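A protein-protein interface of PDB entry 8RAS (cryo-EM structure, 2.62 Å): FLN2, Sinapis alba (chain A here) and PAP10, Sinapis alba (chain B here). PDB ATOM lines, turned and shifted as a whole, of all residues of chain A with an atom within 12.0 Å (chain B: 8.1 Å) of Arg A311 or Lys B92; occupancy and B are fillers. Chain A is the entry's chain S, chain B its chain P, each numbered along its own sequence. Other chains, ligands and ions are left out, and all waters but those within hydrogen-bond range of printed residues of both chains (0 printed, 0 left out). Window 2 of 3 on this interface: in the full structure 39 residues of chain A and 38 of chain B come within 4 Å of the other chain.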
ATOM      1  N   LYS A 307     -13.643 -28.663  15.884  1.00  0.00           N
ATOM      2  CA  LYS A 307     -13.972 -28.270  17.252  1.00  0.00           C
ATOM      3  C   LYS A 307     -12.687 -27.920  17.994  1.00  0.00           C
ATOM      4  O   LYS A 307     -11.923 -28.808  18.385  1.00  0.00           O
ATOM      5  CB  LYS A 307     -14.734 -29.377  17.975  1.00  0.00           C
ATOM      6  CG  LYS A 307     -14.884 -29.145  19.474  1.00  0.00           C
ATOM      7  CD  LYS A 307     -16.135 -28.344  19.797  1.00  0.00           C
ATOM      8  CE  LYS A 307     -16.067 -27.770  21.205  1.00  0.00           C
ATOM      9  NZ  LYS A 307     -16.734 -26.442  21.300  1.00  0.00           N
ATOM     10  N   ILE A 308     -12.466 -26.630  18.205  1.00  0.00           N
ATOM     11  CA  ILE A 308     -11.258 -26.140  18.854  1.00  0.00           C
ATOM     12  C   ILE A 308     -11.466 -26.128  20.362  1.00  0.00           C
ATOM     13  O   ILE A 308     -12.478 -25.615  20.855  1.00  0.00           O
ATOM     14  CB  ILE A 308     -10.890 -24.741  18.338  1.00  0.00           C
ATOM     15  CG1 ILE A 308     -10.600 -24.788  16.837  1.00  0.00           C
ATOM     16  CG2 ILE A 308      -9.709 -24.193  19.108  1.00  0.00           C
ATOM     17  CD1 ILE A 308      -9.981 -23.524  16.296  1.00  0.00           C
ATOM     18  N   SER A 309     -10.511 -26.695  21.094  1.00  0.00           N
ATOM     19  CA  SER A 309     -10.531 -26.650  22.549  1.00  0.00           C
ATOM     20  C   SER A 309      -9.913 -25.338  23.017  1.00  0.00           C
ATOM     21  O   SER A 309      -8.766 -25.031  22.675  1.00  0.00           O
ATOM     22  CB  SER A 309      -9.777 -27.843  23.132  1.00  0.00           C
ATOM     23  OG  SER A 309      -9.831 -27.841  24.548  1.00  0.00           O
ATOM     24  N   LYS A 310     -10.670 -24.565  23.796  1.00  0.00           N
ATOM     25  CA  LYS A 310     -10.252 -23.239  24.231  1.00  0.00           C
ATOM     26  C   LYS A 310      -9.918 -23.196  25.721  1.00  0.00           C
ATOM     27  O   LYS A 310     -10.140 -22.180  26.384  1.00  0.00           O
ATOM     28  CB  LYS A 310     -11.329 -22.207  23.898  1.00  0.00           C
ATOM     29  CG  LYS A 310     -11.626 -22.081  22.413  1.00  0.00           C
ATOM     30  CD  LYS A 310     -11.949 -20.645  22.033  1.00  0.00           C
ATOM     31  CE  LYS A 310     -13.041 -20.070  22.919  1.00  0.00           C
ATOM     32  NZ  LYS A 310     -13.302 -18.635  22.618  1.00  0.00           N
ATOM     33  N   ARG A 311      -9.380 -24.290  26.257  1.00  0.00           N
ATOM     34  CA  ARG A 311      -8.965 -24.357  27.653  1.00  0.00           C
ATOM     35  C   ARG A 311      -7.452 -24.390  27.806  1.00  0.00           C
ATOM     36  O   ARG A 311      -6.883 -23.567  28.528  1.00  0.00           O
ATOM     37  CB  ARG A 311      -9.596 -25.584  28.326  1.00  0.00           C
ATOM     38  CG  ARG A 311     -11.118 -25.557  28.315  1.00  0.00           C
ATOM     39  CD  ARG A 311     -11.718 -26.831  28.887  1.00  0.00           C
ATOM     40  NE  ARG A 311     -13.162 -26.879  28.691  1.00  0.00           N
ATOM     41  CZ  ARG A 311     -13.907 -27.963  28.852  1.00  0.00           C
ATOM     42  NH1 ARG A 311     -13.375 -29.119  29.216  1.00  0.00           N
ATOM     43  NH2 ARG A 311     -15.218 -27.888  28.642  1.00  0.00           N
ATOM     44  N   GLY A 312      -6.785 -25.321  27.141  1.00  0.00           N
ATOM     45  CA  GLY A 312      -5.346 -25.326  27.018  1.00  0.00           C
ATOM     46  C   GLY A 312      -4.906 -24.754  25.689  1.00  0.00           C
ATOM     47  O   GLY A 312      -5.566 -23.881  25.114  1.00  0.00           O
ATOM     48  N   ARG A 313      -3.777 -25.249  25.189  1.00  0.00           N
ATOM     49  CA  ARG A 313      -3.368 -24.898  23.837  1.00  0.00           C
ATOM     50  C   ARG A 313      -4.379 -25.453  22.842  1.00  0.00           C
ATOM     51  O   ARG A 313      -4.928 -26.543  23.030  1.00  0.00           O
ATOM     52  CB  ARG A 313      -1.966 -25.432  23.540  1.00  0.00           C
ATOM     53  CG  ARG A 313      -1.849 -26.946  23.577  1.00  0.00           C
ATOM     54  CD  ARG A 313      -0.504 -27.416  23.049  1.00  0.00           C
ATOM     55  NE  ARG A 313       0.605 -26.862  23.815  1.00  0.00           N
ATOM     56  CZ  ARG A 313       1.060 -27.375  24.950  1.00  0.00           C
ATOM     57  NH1 ARG A 313       0.524 -28.459  25.484  1.00  0.00           N
ATOM     58  NH2 ARG A 313       2.079 -26.781  25.567  1.00  0.00           N
ATOM     59  N   LEU A 314      -4.639 -24.687  21.786  1.00  0.00           N
ATOM     60  CA  LEU A 314      -5.669 -25.061  20.826  1.00  0.00           C
ATOM     61  C   LEU A 314      -5.264 -26.282  20.012  1.00  0.00           C
ATOM     62  O   LEU A 314      -4.249 -26.267  19.308  1.00  0.00           O
ATOM     63  CB  LEU A 314      -5.986 -23.898  19.890  1.00  0.00           C
ATOM     64  CG  LEU A 314      -6.351 -22.498  20.377  1.00  0.00           C
ATOM     65  CD1 LEU A 314      -5.178 -21.649  20.750  1.00  0.00           C
ATOM     66  CD2 LEU A 314      -7.088 -21.858  19.229  1.00  0.00           C
ATOM     67  N   LYS A 315      -6.065 -27.336  20.114  1.00  0.00           N
ATOM     68  CA  LYS A 315      -6.141 -28.374  19.105  1.00  0.00           C
ATOM     69  C   LYS A 315      -7.334 -28.055  18.209  1.00  0.00           C
ATOM     70  O   LYS A 315      -8.008 -27.036  18.376  1.00  0.00           O
ATOM     71  CB  LYS A 315      -6.253 -29.754  19.754  1.00  0.00           C
ATOM     72  CG  LYS A 315      -5.032 -30.638  19.537  1.00  0.00           C
ATOM     73  CD  LYS A 315      -3.808 -30.112  20.277  1.00  0.00           C
ATOM     74  CE  LYS A 315      -3.727 -30.687  21.685  1.00  0.00           C
ATOM     75  NZ  LYS A 315      -2.636 -30.078  22.499  1.00  0.00           N
ATOM     76  N   SER A 316      -7.604 -28.923  17.238  1.00  0.00           N
ATOM     77  CA  SER A 316      -8.700 -28.622  16.328  1.00  0.00           C
ATOM     78  C   SER A 316      -9.724 -29.750  16.263  1.00  0.00           C
ATOM     79  O   SER A 316     -10.907 -29.490  16.023  1.00  0.00           O
ATOM     80  CB  SER A 316      -8.155 -28.294  14.939  1.00  0.00           C
ATOM     81  OG  SER A 316      -7.411 -29.373  14.416  1.00  0.00           O
ATOM     82  N   THR A 317      -9.283 -30.993  16.461  1.00  0.00           N
ATOM     83  CA  THR A 317     -10.168 -32.129  16.733  1.00  0.00           C
ATOM     84  C   THR A 317     -11.307 -32.219  15.711  1.00  0.00           C
ATOM     85  O   THR A 317     -12.473 -31.966  16.012  1.00  0.00           O
ATOM     86  CB  THR A 317     -10.724 -32.055  18.159  1.00  0.00           C
ATOM     87  OG1 THR A 317     -11.781 -31.089  18.215  1.00  0.00           O
ATOM     88  CG2 THR A 317      -9.629 -31.669  19.145  1.00  0.00           C
ATOM     89  N   GLN B  85       1.867 -17.984  19.812  1.00  0.00           N
ATOM     90  CA  GLN B  85       1.347 -17.472  21.077  1.00  0.00           C
ATOM     91  C   GLN B  85       0.388 -16.306  20.867  1.00  0.00           C
ATOM     92  O   GLN B  85      -0.570 -16.146  21.635  1.00  0.00           O
ATOM     93  CB  GLN B  85       2.496 -17.055  21.995  1.00  0.00           C
ATOM     94  CG  GLN B  85       3.519 -16.142  21.346  1.00  0.00           C
ATOM     95  CD  GLN B  85       4.759 -16.886  20.895  1.00  0.00           C
ATOM     96  OE1 GLN B  85       4.742 -18.108  20.741  1.00  0.00           O
ATOM     97  NE2 GLN B  85       5.844 -16.151  20.675  1.00  0.00           N
ATOM     98  N   GLU B  86       0.623 -15.477  19.851  1.00  0.00           N
ATOM     99  CA  GLU B  86      -0.303 -14.381  19.598  1.00  0.00           C
ATOM    100  C   GLU B  86      -1.658 -14.908  19.137  1.00  0.00           C
ATOM    101  O   GLU B  86      -2.700 -14.373  19.524  1.00  0.00           O
ATOM    102  CB  GLU B  86       0.279 -13.411  18.573  1.00  0.00           C
ATOM    103  CG  GLU B  86      -0.220 -11.985  18.750  1.00  0.00           C
ATOM    104  CD  GLU B  86      -1.573 -11.749  18.115  1.00  0.00           C
ATOM    105  OE1 GLU B  86      -2.551 -11.520  18.857  1.00  0.00           O
ATOM    106  OE2 GLU B  86      -1.660 -11.788  16.875  1.00  0.00           O
ATOM    107  N   LEU B  87      -1.663 -15.962  18.316  1.00  0.00           N
ATOM    108  CA  LEU B  87      -2.920 -16.611  17.956  1.00  0.00           C
ATOM    109  C   LEU B  87      -3.560 -17.277  19.166  1.00  0.00           C
ATOM    110  O   LEU B  87      -4.792 -17.291  19.298  1.00  0.00           O
ATOM    111  CB  LEU B  87      -2.689 -17.631  16.842  1.00  0.00           C
ATOM    112  CG  LEU B  87      -3.906 -17.987  15.984  1.00  0.00           C
ATOM    113  CD1 LEU B  87      -4.597 -16.732  15.473  1.00  0.00           C
ATOM    114  CD2 LEU B  87      -3.501 -18.883  14.828  1.00  0.00           C
ATOM    115  N   GLN B  88      -2.735 -17.843  20.053  1.00  0.00           N
ATOM    116  CA  GLN B  88      -3.234 -18.391  21.309  1.00  0.00           C
ATOM    117  C   GLN B  88      -4.048 -17.328  22.036  1.00  0.00           C
ATOM    118  O   GLN B  88      -5.207 -17.544  22.412  1.00  0.00           O
ATOM    119  CB  GLN B  88      -2.062 -18.814  22.203  1.00  0.00           C
ATOM    120  CG  GLN B  88      -1.818 -20.303  22.446  1.00  0.00           C
ATOM    121  CD  GLN B  88      -1.308 -21.033  21.210  1.00  0.00           C
ATOM    122  OE1 GLN B  88      -0.131 -20.929  20.873  1.00  0.00           O
ATOM    123  NE2 GLN B  88      -2.167 -21.794  20.563  1.00  0.00           N
ATOM    124  N   ASP B  89      -3.440 -16.152  22.212  1.00  0.00           N
ATOM    125  CA  ASP B  89      -4.090 -15.042  22.904  1.00  0.00           C
ATOM    126  C   ASP B  89      -5.341 -14.588  22.163  1.00  0.00           C
ATOM    127  O   ASP B  89      -6.389 -14.355  22.777  1.00  0.00           O
ATOM    128  CB  ASP B  89      -3.100 -13.883  23.056  1.00  0.00           C
ATOM    129  CG  ASP B  89      -3.773 -12.575  23.447  1.00  0.00           C
ATOM    130  OD1 ASP B  89      -4.733 -12.600  24.246  1.00  0.00           O
ATOM    131  OD2 ASP B  89      -3.338 -11.514  22.950  1.00  0.00           O
ATOM    132  N   LEU B  90      -5.251 -14.463  20.836  1.00  0.00           N
ATOM    133  CA  LEU B  90      -6.369 -13.937  20.061  1.00  0.00           C
ATOM    134  C   LEU B  90      -7.591 -14.840  20.175  1.00  0.00           C
ATOM    135  O   LEU B  90      -8.710 -14.354  20.380  1.00  0.00           O
ATOM    136  CB  LEU B  90      -5.953 -13.764  18.598  1.00  0.00           C
ATOM    137  CG  LEU B  90      -6.720 -12.821  17.655  1.00  0.00           C
ATOM    138  CD1 LEU B  90      -8.166 -13.244  17.404  1.00  0.00           C
ATOM    139  CD2 LEU B  90      -6.666 -11.392  18.177  1.00  0.00           C
ATOM    140  N   VAL B  91      -7.405 -16.154  20.041  1.00  0.00           N
ATOM    141  CA  VAL B  91      -8.552 -17.051  20.141  1.00  0.00           C
ATOM    142  C   VAL B  91      -9.042 -17.134  21.582  1.00  0.00           C
ATOM    143  O   VAL B  91     -10.253 -17.107  21.839  1.00  0.00           O
ATOM    144  CB  VAL B  91      -8.218 -18.441  19.576  1.00  0.00           C
ATOM    145  CG1 VAL B  91      -9.446 -19.339  19.665  1.00  0.00           C
ATOM    146  CG2 VAL B  91      -7.736 -18.327  18.141  1.00  0.00           C
ATOM    147  N   LYS B  92      -8.120 -17.236  22.546  1.00  0.00           N
ATOM    148  CA  LYS B  92      -8.536 -17.273  23.944  1.00  0.00           C
ATOM    149  C   LYS B  92      -9.203 -15.976  24.382  1.00  0.00           C
ATOM    150  O   LYS B  92      -9.961 -15.982  25.358  1.00  0.00           O
ATOM    151  CB  LYS B  92      -7.343 -17.585  24.848  1.00  0.00           C
ATOM    152  CG  LYS B  92      -6.842 -19.013  24.724  1.00  0.00           C
ATOM    153  CD  LYS B  92      -5.845 -19.349  25.817  1.00  0.00           C
ATOM    154  CE  LYS B  92      -5.260 -20.734  25.614  1.00  0.00           C
ATOM    155  NZ  LYS B  92      -4.745 -21.309  26.887  1.00  0.00           N
ATOM    156  N   GLY B  93      -8.945 -14.873  23.686  1.00  0.00           N
ATOM    157  CA  GLY B  93      -9.651 -13.632  23.923  1.00  0.00           C
ATOM    158  C   GLY B  93     -11.033 -13.661  23.305  1.00  0.00           C
ATOM    159  O   GLY B  93     -11.610 -14.720  23.044  1.00  0.00           O
ATOM    160  N   GLU B  94     -11.573 -12.469  23.066  1.00  0.00           N
ATOM    161  CA  GLU B  94     -12.898 -12.336  22.484  1.00  0.00           C
ATOM    162  C   GLU B  94     -12.871 -11.287  21.383  1.00  0.00           C
ATOM    163  O   GLU B  94     -12.079 -10.342  21.420  1.00  0.00           O
ATOM    164  CB  GLU B  94     -13.944 -11.965  23.544  1.00  0.00           C
ATOM    165  CG  GLU B  94     -14.570 -13.169  24.228  1.00  0.00           C
ATOM    166  CD  GLU B  94     -15.392 -12.790  25.443  1.00  0.00           C
ATOM    167  OE1 GLU B  94     -15.127 -11.720  26.033  1.00  0.00           O
ATOM    168  OE2 GLU B  94     -16.303 -13.562  25.810  1.00  0.00           O
ATOM    169  N   ARG B  95     -13.747 -11.470  20.397  1.00  0.00           N
ATOM    170  CA  ARG B  95     -13.849 -10.551  19.275  1.00  0.00           C
ATOM    171  C   ARG B  95     -15.266 -10.596  18.725  1.00  0.00           C
ATOM    172  O   ARG B  95     -15.990 -11.579  18.902  1.00  0.00           O
ATOM    173  CB  ARG B  95     -12.833 -10.887  18.176  1.00  0.00           C
ATOM    174  CG  ARG B  95     -13.133 -12.175  17.429  1.00  0.00           C
ATOM    175  CD  ARG B  95     -11.860 -12.942  17.112  1.00  0.00           C
ATOM    176  NE  ARG B  95     -11.531 -13.916  18.147  1.00  0.00           N
ATOM    177  CZ  ARG B  95     -12.097 -15.111  18.260  1.00  0.00           C
ATOM    178  NH1 ARG B  95     -13.031 -15.516  17.416  1.00  0.00           N
ATOM    179  NH2 ARG B  95     -11.713 -15.919  19.243  1.00  0.00           N
ATOM    180  N   LEU B  99     -12.658 -14.269  12.343  1.00  0.00           N
ATOM    181  CA  LEU B  99     -11.208 -14.343  12.244  1.00  0.00           C
ATOM    182  C   LEU B  99     -10.842 -15.435  11.251  1.00  0.00           C
ATOM    183  O   LEU B  99     -11.262 -16.586  11.406  1.00  0.00           O
ATOM    184  CB  LEU B  99     -10.579 -14.621  13.609  1.00  0.00           C
ATOM    185  CG  LEU B  99      -9.156 -15.176  13.583  1.00  0.00           C
ATOM    186  CD1 LEU B  99      -8.157 -14.066  13.315  1.00  0.00           C
ATOM    187  CD2 LEU B  99      -8.833 -15.892  14.886  1.00  0.00           C
ATOM    188  N   ILE B 157     -12.531 -18.944  12.160  1.00  0.00           N
ATOM    189  CA  ILE B 157     -12.818 -19.041  13.587  1.00  0.00           C
ATOM    190  C   ILE B 157     -14.047 -18.195  13.884  1.00  0.00           C
ATOM    191  O   ILE B 157     -14.057 -16.986  13.628  1.00  0.00           O
ATOM    192  CB  ILE B 157     -11.619 -18.587  14.433  1.00  0.00           C
ATOM    193  CG1 ILE B 157     -10.331 -19.229  13.914  1.00  0.00           C
ATOM    194  CG2 ILE B 157     -11.838 -18.942  15.892  1.00  0.00           C
ATOM    195  CD1 ILE B 157     -10.306 -20.732  14.032  1.00  0.00           C
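O of Val B91 is in hydrogen-bond range of NH2 of Arg B95, 3.2 Å away.
The backbone carbonyl oxygen (O) of Leu B99 lies within hydrogen-bond range of the backbone NH (N) of Ile B157 (2.8 Å).
Among the printed residues, pairs that only touch across the chains: Ile A308 with Ile B157, Arg A311 with Lys B92, Leu A314 with Gln B88 and Leu A314 with Val B91.
Of the 11 printed residues of chain A, 5 touch a printed residue of chain B.
Hydrophobic or aromatic side chains of chain A within 4 Å of the printed part of chain B: Ile A308 and Leu A314.
Of the 13 printed residues of chain B, 4 touch a printed residue of chain A.
Hydrophobic or aromatic side chains of chain B within 4 Å of the printed part of chain A: Val B91 and Ile B157.
Among the printed residues, 6 pairs touch across the chains.
Among the printed residues, no Asp or Glu carboxylate lies within 4 Å of a Lys or Arg side-chain nitrogen of the other chain.
The backbone carbonyl oxygen of Gly A312 sits close to the side-chain amino group of Lys B92, 3.2 Å away.
The side-chain amino group (NZ) of Lys A310 is in hydrogen-bond range of the backbone carbonyl oxygen (O) of Val B91.
Printed residues of chain B within 4 Å of Ile A308: Ile B157.
Of the printed residues of chain B, Lys A310 touches Val B91 (3.5 Å).
Arg A311 touches just one residue of chain B: Lys B92 (3.5 Å).
Gly A312 touches just one residue of chain B: Lys B92.
Of the printed residues of chain B, Leu A314 touches Gln B88 and Val B91.
Of chain A, only Leu A314 comes within 4 Å of Gln B88.
No residue of chain A comes within 4 Å of Asp B89.
No residue of chain A comes within 4 Å of Leu B90.
Val B91 touches two residues of chain A.
Lys B92 touches just these residues of chain A: Arg A311 and Gly A312.
No residue of chain A comes within 4 Å of Gly B93.
The nearest residue of chain A that does not touch Lys B92 is Arg A313 (4.4 Å).
The nearest printed residue of chain B that does not touch Lys A310 is Gly B93 (4.3 Å).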
